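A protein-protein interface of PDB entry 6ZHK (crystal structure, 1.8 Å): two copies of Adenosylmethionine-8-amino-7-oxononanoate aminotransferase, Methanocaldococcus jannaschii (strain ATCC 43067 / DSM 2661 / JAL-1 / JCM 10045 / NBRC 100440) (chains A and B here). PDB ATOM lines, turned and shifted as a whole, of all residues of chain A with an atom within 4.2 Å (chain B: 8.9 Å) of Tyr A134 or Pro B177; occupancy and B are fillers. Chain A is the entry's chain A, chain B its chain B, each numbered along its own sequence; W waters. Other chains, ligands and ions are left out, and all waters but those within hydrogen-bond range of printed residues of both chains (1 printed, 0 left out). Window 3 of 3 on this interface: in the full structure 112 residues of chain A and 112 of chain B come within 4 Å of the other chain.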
ATOM      1  N   ILE A 130      27.360   9.668   6.061  1.00  0.00           N
ATOM      2  CA  ILE A 130      27.883   9.166   4.788  1.00  0.00           C
ATOM      3  C   ILE A 130      26.717   9.030   3.799  1.00  0.00           C
ATOM      4  O   ILE A 130      26.850   9.425   2.639  1.00  0.00           O
ATOM      5  CB  ILE A 130      28.654   7.820   5.007  1.00  0.00           C
ATOM      6  CG1 ILE A 130      30.036   8.070   5.607  1.00  0.00           C
ATOM      7  CG2 ILE A 130      28.732   6.942   3.749  1.00  0.00           C
ATOM      8  CD1 ILE A 130      30.677   6.738   6.122  1.00  0.00           C
ATOM      9  N   LYS A 131      25.622   8.386   4.231  1.00  0.00           N
ATOM     10  CA  LYS A 131      24.533   8.043   3.337  1.00  0.00           C
ATOM     11  C   LYS A 131      23.800   9.293   2.894  1.00  0.00           C
ATOM     12  O   LYS A 131      23.434   9.405   1.731  1.00  0.00           O
ATOM     13  CB  LYS A 131      23.592   6.993   3.916  1.00  0.00           C
ATOM     14  CG  LYS A 131      24.269   5.642   4.201  1.00  0.00           C
ATOM     15  CD  LYS A 131      23.299   4.674   4.839  1.00  0.00           C
ATOM     16  CE  LYS A 131      21.920   4.614   4.163  1.00  0.00           C
ATOM     17  NZ  LYS A 131      21.084   3.541   4.778  1.00  0.00           N
ATOM     18  N   MET A 132      23.664  10.278   3.795  1.00  0.00           N
ATOM     19  CA  MET A 132      23.006  11.525   3.454  1.00  0.00           C
ATOM     20  C   MET A 132      23.835  12.227   2.383  1.00  0.00           C
ATOM     21  O   MET A 132      23.248  12.731   1.427  1.00  0.00           O
ATOM     22  CB  MET A 132      22.941  12.421   4.715  1.00  0.00           C
ATOM     23  CG  MET A 132      21.872  11.964   5.693  1.00  0.00           C
ATOM     24  SD  MET A 132      22.062  13.007   7.137  1.00  0.00           S
ATOM     25  CE  MET A 132      20.575  12.604   8.053  1.00  0.00           C
ATOM     26  N   ALA A 133      25.169  12.269   2.562  1.00  0.00           N
ATOM     27  CA  ALA A 133      26.060  13.010   1.675  1.00  0.00           C
ATOM     28  C   ALA A 133      26.013  12.343   0.295  1.00  0.00           C
ATOM     29  O   ALA A 133      25.766  12.994  -0.692  1.00  0.00           O
ATOM     30  CB  ALA A 133      27.481  13.075   2.215  1.00  0.00           C
ATOM     31  N   TYR A 134      26.055  10.997   0.300  1.00  0.00           N
ATOM     32  CA  TYR A 134      26.074  10.237  -0.942  1.00  0.00           C
ATOM     33  C   TYR A 134      24.765  10.491  -1.689  1.00  0.00           C
ATOM     34  O   TYR A 134      24.755  10.784  -2.919  1.00  0.00           O
ATOM     35  CB  TYR A 134      26.284   8.737  -0.686  1.00  0.00           C
ATOM     36  CG  TYR A 134      26.285   7.970  -2.009  1.00  0.00           C
ATOM     37  CD1 TYR A 134      27.433   7.948  -2.800  1.00  0.00           C
ATOM     38  CD2 TYR A 134      25.131   7.351  -2.501  1.00  0.00           C
ATOM     39  CE1 TYR A 134      27.446   7.294  -4.037  1.00  0.00           C
ATOM     40  CE2 TYR A 134      25.127   6.744  -3.739  1.00  0.00           C
ATOM     41  CZ  TYR A 134      26.282   6.698  -4.492  1.00  0.00           C
ATOM     42  OH  TYR A 134      26.280   6.091  -5.730  1.00  0.00           O
ATOM     43  N   GLN A 135      23.659  10.312  -0.959  1.00  0.00           N
ATOM     44  CA  GLN A 135      22.360  10.380  -1.625  1.00  0.00           C
ATOM     45  C   GLN A 135      21.984  11.812  -1.965  1.00  0.00           C
ATOM     46  O   GLN A 135      21.334  12.045  -2.992  1.00  0.00           O
ATOM     47  CB  GLN A 135      21.285   9.610  -0.862  1.00  0.00           C
ATOM     48  CG  GLN A 135      19.951   9.650  -1.611  1.00  0.00           C
ATOM     49  CD  GLN A 135      18.993   8.670  -1.008  1.00  0.00           C
ATOM     50  OE1 GLN A 135      19.150   8.241   0.138  1.00  0.00           O
ATOM     51  NE2 GLN A 135      17.899   8.450  -1.724  1.00  0.00           N
ATOM     52  N   TYR A 136      22.480  12.778  -1.182  1.00  0.00           N
ATOM     53  CA  TYR A 136      22.277  14.175  -1.557  1.00  0.00           C
ATOM     54  C   TYR A 136      22.691  14.392  -3.020  1.00  0.00           C
ATOM     55  O   TYR A 136      21.952  14.999  -3.815  1.00  0.00           O
ATOM     56  CB  TYR A 136      23.109  15.081  -0.664  1.00  0.00           C
ATOM     57  CG  TYR A 136      23.222  16.528  -1.092  1.00  0.00           C
ATOM     58  CD1 TYR A 136      22.187  17.451  -0.871  1.00  0.00           C
ATOM     59  CD2 TYR A 136      24.370  16.975  -1.719  1.00  0.00           C
ATOM     60  CE1 TYR A 136      22.337  18.812  -1.211  1.00  0.00           C
ATOM     61  CE2 TYR A 136      24.516  18.322  -2.076  1.00  0.00           C
ATOM     62  CZ  TYR A 136      23.484  19.216  -1.866  1.00  0.00           C
ATOM     63  OH  TYR A 136      23.672  20.550  -2.183  1.00  0.00           O
ATOM     64  N   TYR A 137      23.907  13.966  -3.373  1.00  0.00           N
ATOM     65  CA  TYR A 137      24.415  14.280  -4.702  1.00  0.00           C
ATOM     66  C   TYR A 137      23.675  13.476  -5.762  1.00  0.00           C
ATOM     67  O   TYR A 137      23.429  13.982  -6.847  1.00  0.00           O
ATOM     68  CB  TYR A 137      25.922  14.027  -4.821  1.00  0.00           C
ATOM     69  CG  TYR A 137      26.747  15.048  -4.068  1.00  0.00           C
ATOM     70  CD1 TYR A 137      26.824  16.363  -4.516  1.00  0.00           C
ATOM     71  CD2 TYR A 137      27.415  14.710  -2.884  1.00  0.00           C
ATOM     72  CE1 TYR A 137      27.594  17.317  -3.850  1.00  0.00           C
ATOM     73  CE2 TYR A 137      28.187  15.661  -2.227  1.00  0.00           C
ATOM     74  CZ  TYR A 137      28.278  16.955  -2.697  1.00  0.00           C
ATOM     75  OH  TYR A 137      29.031  17.865  -1.999  1.00  0.00           O
ATOM     76  N   VAL A 138      23.278  12.232  -5.448  1.00  0.00           N
ATOM     77  CA  VAL A 138      22.487  11.527  -6.433  1.00  0.00           C
ATOM     78  C   VAL A 138      21.203  12.310  -6.722  1.00  0.00           C
ATOM     79  O   VAL A 138      20.763  12.432  -7.887  1.00  0.00           O
ATOM     80  CB  VAL A 138      22.125  10.139  -5.888  1.00  0.00           C
ATOM     81  CG1 VAL A 138      21.041   9.506  -6.730  1.00  0.00           C
ATOM     82  CG2 VAL A 138      23.359   9.254  -5.775  1.00  0.00           C
ATOM     83  N   ARG A 145      29.873  10.734  -7.917  1.00  0.00           N
ATOM     84  CA  ARG A 145      30.463  11.123  -6.631  1.00  0.00           C
ATOM     85  C   ARG A 145      30.354   9.979  -5.617  1.00  0.00           C
ATOM     86  O   ARG A 145      29.424   9.971  -4.793  1.00  0.00           O
ATOM     87  CB  ARG A 145      29.693  12.313  -6.041  1.00  0.00           C
ATOM     88  CG  ARG A 145      29.658  13.547  -6.925  1.00  0.00           C
ATOM     89  CD  ARG A 145      30.480  14.504  -6.118  1.00  0.00           C
ATOM     90  NE  ARG A 145      30.033  15.791  -6.523  1.00  0.00           N
ATOM     91  CZ  ARG A 145      30.403  16.929  -5.989  1.00  0.00           C
ATOM     92  NH1 ARG A 145      31.170  16.968  -4.899  1.00  0.00           N
ATOM     93  NH2 ARG A 145      29.878  18.013  -6.520  1.00  0.00           N
ATOM     94  N   THR A 146      31.305   9.049  -5.713  1.00  0.00           N
ATOM     95  CA  THR A 146      31.248   7.757  -5.056  1.00  0.00           C
ATOM     96  C   THR A 146      32.422   7.579  -4.098  1.00  0.00           C
ATOM     97  O   THR A 146      32.448   6.622  -3.335  1.00  0.00           O
ATOM     98  CB  THR A 146      31.240   6.613  -6.071  1.00  0.00           C
ATOM     99  OG1 THR A 146      32.454   6.706  -6.790  1.00  0.00           O
ATOM    100  CG2 THR A 146      30.123   6.727  -7.081  1.00  0.00           C
ATOM    101  N   PHE A 229      31.873  12.491  -2.508  1.00  0.00           N
ATOM    102  CA  PHE A 229      30.632  12.916  -1.849  1.00  0.00           C
ATOM    103  C   PHE A 229      30.830  13.532  -0.463  1.00  0.00           C
ATOM    104  O   PHE A 229      29.896  14.171   0.060  1.00  0.00           O
ATOM    105  CB  PHE A 229      29.584  11.800  -1.827  1.00  0.00           C
ATOM    106  CG  PHE A 229      30.020  10.602  -1.029  1.00  0.00           C
ATOM    107  CD1 PHE A 229      29.837  10.606   0.355  1.00  0.00           C
ATOM    108  CD2 PHE A 229      30.685   9.534  -1.620  1.00  0.00           C
ATOM    109  CE1 PHE A 229      30.237   9.505   1.122  1.00  0.00           C
ATOM    110  CE2 PHE A 229      31.037   8.418  -0.859  1.00  0.00           C
ATOM    111  CZ  PHE A 229      30.817   8.396   0.513  1.00  0.00           C
ATOM    112  N   VAL B 160      26.237   0.208   6.355  1.00  0.00           N
ATOM    113  CA  VAL B 160      26.754  -0.255   5.049  1.00  0.00           C
ATOM    114  C   VAL B 160      26.923  -1.780   4.998  1.00  0.00           C
ATOM    115  O   VAL B 160      26.608  -2.422   3.992  1.00  0.00           O
ATOM    116  CB  VAL B 160      28.010   0.515   4.647  1.00  0.00           C
ATOM    117  CG1 VAL B 160      28.695  -0.098   3.450  1.00  0.00           C
ATOM    118  CG2 VAL B 160      27.645   1.966   4.324  1.00  0.00           C
ATOM    119  N   MET B 163      23.456  -3.303   4.881  1.00  0.00           N
ATOM    120  CA  MET B 163      22.799  -3.095   3.598  1.00  0.00           C
ATOM    121  C   MET B 163      23.413  -4.055   2.558  1.00  0.00           C
ATOM    122  O   MET B 163      22.681  -4.555   1.701  1.00  0.00           O
ATOM    123  CB  MET B 163      22.979  -1.670   3.048  1.00  0.00           C
ATOM    124  CG  MET B 163      22.177  -0.615   3.808  1.00  0.00           C
ATOM    125  SD  MET B 163      22.235   0.981   2.921  1.00  0.00           S
ATOM    126  CE  MET B 163      23.941   1.467   3.173  1.00  0.00           C
ATOM    127  N   SER B 164      24.732  -4.301   2.625  1.00  0.00           N
ATOM    128  CA  SER B 164      25.423  -5.142   1.639  1.00  0.00           C
ATOM    129  C   SER B 164      24.813  -6.540   1.652  1.00  0.00           C
ATOM    130  O   SER B 164      24.571  -7.120   0.577  1.00  0.00           O
ATOM    131  CB  SER B 164      26.958  -5.242   1.870  1.00  0.00           C
ATOM    132  OG  SER B 164      27.488  -3.899   1.815  1.00  0.00           O
ATOM    133  N   HIS B 172      17.846   0.341  -0.266  1.00  0.00           N
ATOM    134  CA  HIS B 172      19.309   0.427  -0.192  1.00  0.00           C
ATOM    135  C   HIS B 172      19.964   0.456  -1.578  1.00  0.00           C
ATOM    136  O   HIS B 172      21.147   0.729  -1.655  1.00  0.00           O
ATOM    137  CB  HIS B 172      19.831  -0.806   0.562  1.00  0.00           C
ATOM    138  CG  HIS B 172      19.311  -0.892   1.955  1.00  0.00           C
ATOM    139  ND1 HIS B 172      19.091  -2.120   2.568  1.00  0.00           N
ATOM    140  CD2 HIS B 172      19.023   0.064   2.850  1.00  0.00           C
ATOM    141  CE1 HIS B 172      18.656  -1.886   3.803  1.00  0.00           C
ATOM    142  NE2 HIS B 172      18.630  -0.564   4.010  1.00  0.00           N
ATOM    143  N   GLY B 173      19.159   0.295  -2.657  1.00  0.00           N
ATOM    144  CA  GLY B 173      19.664   0.088  -4.017  1.00  0.00           C
ATOM    145  C   GLY B 173      20.530   1.262  -4.475  1.00  0.00           C
ATOM    146  O   GLY B 173      21.476   1.106  -5.230  1.00  0.00           O
ATOM    147  N   VAL B 174      20.116   2.470  -4.110  1.00  0.00           N
ATOM    148  CA  VAL B 174      20.883   3.644  -4.475  1.00  0.00           C
ATOM    149  C   VAL B 174      22.337   3.627  -3.952  1.00  0.00           C
ATOM    150  O   VAL B 174      23.237   4.275  -4.481  1.00  0.00           O
ATOM    151  CB  VAL B 174      20.071   4.868  -4.036  1.00  0.00           C
ATOM    152  CG1 VAL B 174      20.020   5.005  -2.511  1.00  0.00           C
ATOM    153  CG2 VAL B 174      20.604   6.148  -4.688  1.00  0.00           C
ATOM    154  N   PHE B 175      22.597   2.887  -2.863  1.00  0.00           N
ATOM    155  CA  PHE B 175      23.911   2.906  -2.233  1.00  0.00           C
ATOM    156  C   PHE B 175      24.845   1.854  -2.827  1.00  0.00           C
ATOM    157  O   PHE B 175      25.930   1.668  -2.287  1.00  0.00           O
ATOM    158  CB  PHE B 175      23.737   2.742  -0.711  1.00  0.00           C
ATOM    159  CG  PHE B 175      23.006   3.921  -0.132  1.00  0.00           C
ATOM    160  CD1 PHE B 175      23.647   5.169  -0.036  1.00  0.00           C
ATOM    161  CD2 PHE B 175      21.694   3.784   0.276  1.00  0.00           C
ATOM    162  CE1 PHE B 175      22.944   6.267   0.414  1.00  0.00           C
ATOM    163  CE2 PHE B 175      21.004   4.866   0.799  1.00  0.00           C
ATOM    164  CZ  PHE B 175      21.619   6.119   0.809  1.00  0.00           C
ATOM    165  N   LYS B 176      24.468   1.212  -3.959  1.00  0.00           N
ATOM    166  CA  LYS B 176      25.217   0.055  -4.481  1.00  0.00           C
ATOM    167  C   LYS B 176      26.727   0.299  -4.625  1.00  0.00           C
ATOM    168  O   LYS B 176      27.515  -0.563  -4.280  1.00  0.00           O
ATOM    169  CB  LYS B 176      24.604  -0.529  -5.765  1.00  0.00           C
ATOM    170  CG  LYS B 176      23.453  -1.530  -5.582  1.00  0.00           C
ATOM    171  CD  LYS B 176      23.253  -2.344  -6.885  1.00  0.00           C
ATOM    172  CE  LYS B 176      21.932  -3.087  -7.017  1.00  0.00           C
ATOM    173  NZ  LYS B 176      21.021  -2.458  -8.010  1.00  0.00           N
ATOM    174  N   PRO B 177      27.225   1.474  -5.078  1.00  0.00           N
ATOM    175  CA  PRO B 177      28.667   1.721  -5.140  1.00  0.00           C
ATOM    176  C   PRO B 177      29.394   1.585  -3.796  1.00  0.00           C
ATOM    177  O   PRO B 177      30.597   1.284  -3.777  1.00  0.00           O
ATOM    178  CB  PRO B 177      28.715   3.192  -5.615  1.00  0.00           C
ATOM    179  CG  PRO B 177      27.502   3.195  -6.528  1.00  0.00           C
ATOM    180  CD  PRO B 177      26.429   2.579  -5.663  1.00  0.00           C
ATOM    181  N   LEU B 178      28.656   1.726  -2.691  1.00  0.00           N
ATOM    182  CA  LEU B 178      29.301   1.638  -1.370  1.00  0.00           C
ATOM    183  C   LEU B 178      29.221   0.228  -0.769  1.00  0.00           C
ATOM    184  O   LEU B 178      29.861  -0.054   0.234  1.00  0.00           O
ATOM    185  CB  LEU B 178      28.650   2.604  -0.391  1.00  0.00           C
ATOM    186  CG  LEU B 178      28.554   4.072  -0.823  1.00  0.00           C
ATOM    187  CD1 LEU B 178      27.950   4.872   0.337  1.00  0.00           C
ATOM    188  CD2 LEU B 178      29.951   4.578  -1.181  1.00  0.00           C
ATOM    189  N   LEU B 179      28.469  -0.662  -1.401  1.00  0.00           N
ATOM    190  CA  LEU B 179      28.239  -1.969  -0.798  1.00  0.00           C
ATOM    191  C   LEU B 179      29.246  -3.003  -1.300  1.00  0.00           C
ATOM    192  O   LEU B 179      29.632  -2.983  -2.480  1.00  0.00           O
ATOM    193  CB  LEU B 179      26.836  -2.426  -1.196  1.00  0.00           C
ATOM    194  CG  LEU B 179      25.721  -1.412  -0.914  1.00  0.00           C
ATOM    195  CD1 LEU B 179      24.370  -2.071  -1.268  1.00  0.00           C
ATOM    196  CD2 LEU B 179      25.740  -0.941   0.558  1.00  0.00           C
ATOM    197  N   PHE B 180      29.606  -3.935  -0.403  1.00  0.00           N
ATOM    198  CA  PHE B 180      30.458  -5.012  -0.862  1.00  0.00           C
ATOM    199  C   PHE B 180      29.537  -6.091  -1.457  1.00  0.00           C
ATOM    200  O   PHE B 180      28.362  -6.164  -1.101  1.00  0.00           O
ATOM    201  CB  PHE B 180      31.364  -5.524   0.267  1.00  0.00           C
ATOM    202  CG  PHE B 180      30.639  -6.018   1.502  1.00  0.00           C
ATOM    203  CD1 PHE B 180      30.086  -7.293   1.543  1.00  0.00           C
ATOM    204  CD2 PHE B 180      30.600  -5.262   2.657  1.00  0.00           C
ATOM    205  CE1 PHE B 180      29.458  -7.789   2.683  1.00  0.00           C
ATOM    206  CE2 PHE B 180      29.979  -5.738   3.802  1.00  0.00           C
ATOM    207  CZ  PHE B 180      29.429  -7.028   3.828  1.00  0.00           C
ATOM    208  N   LYS B 181      30.058  -6.856  -2.431  1.00  0.00           N
ATOM    209  CA  LYS B 181      29.187  -7.659  -3.279  1.00  0.00           C
ATOM    210  C   LYS B 181      29.194  -9.115  -2.817  1.00  0.00           C
ATOM    211  O   LYS B 181      30.159  -9.652  -2.272  1.00  0.00           O
ATOM    212  CB  LYS B 181      29.589  -7.464  -4.758  1.00  0.00           C
ATOM    213  CG  LYS B 181      29.544  -6.002  -5.279  1.00  0.00           C
ATOM    214  CD  LYS B 181      28.167  -5.345  -5.036  1.00  0.00           C
ATOM    215  CE  LYS B 181      27.916  -3.920  -5.529  1.00  0.00           C
ATOM    216  NZ  LYS B 181      28.960  -2.958  -5.131  1.00  0.00           N
HETATM  217  O   HOH W   1      24.007   5.331  -6.780  1.00  0.00           O
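Printed residues of chain A that touch a printed residue of chain B: Lys A131, Tyr A134, Gln A135, Val A138 and Thr A146. Along chain A the printed residues that touch a printed residue of chain B span positions 131 to 146. Among the printed residues, 8 pairs touch across the chains.
The side-chain amino group of Lys A131 sits at hydrogen-bond distance from the side-chain sulfur of Met B163, 3.4 Å away.
No position is printed for both chains.
Water W1 bridges the side-chain hydroxyl (OH) of Tyr A134 (2.6 Å) and the backbone carbonyl oxygen (O) of Val B174 (2.6 Å).
Phe B175 touches Lys A131 (CE1 to O, 3.4 Å). Val B174 touches Tyr A134 (O to CE2, 3.2 Å). Phe B175 touches Tyr A134 (CD1 to CD2, 3.6 Å). Pro B177 touches Tyr A134 (CG to OH, 3.2 Å). Phe B175 touches Gln A135. Val A138 touches Val B174. CD2 of Leu B178 touches O of Thr A146, 3.9 Å away.
No residue of chain B comes within 4 Å of Ala A133. Tyr A134 touches just these residues of chain B: Val B174 (3.2 Å), Phe B175 (3.6 Å) and Pro B177 (3.2 Å). Printed residues of chain B within 4 Å of Gln A135: Phe B175 (3.3 Å). Of the printed residues of chain B, Thr A146 touches Leu B178. Printed residues of chain A within 4 Å of Val B174: Tyr A134 and Val A138. Printed residues of chain A within 4 Å of Phe B175: Lys A131 (3.4 Å), Tyr A134 (3.6 Å) and Gln A135 (3.3 Å). Pro B177 touches one residue of chain A. Printed residues of chain A within 4 Å of Leu B178: Thr A146. The nearest residue of chain A that does not touch Pro B177 is Thr A146 (4.1 Å). The nearest printed residue of chain B that does not touch Lys A131 is His B172 (4.5 Å).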
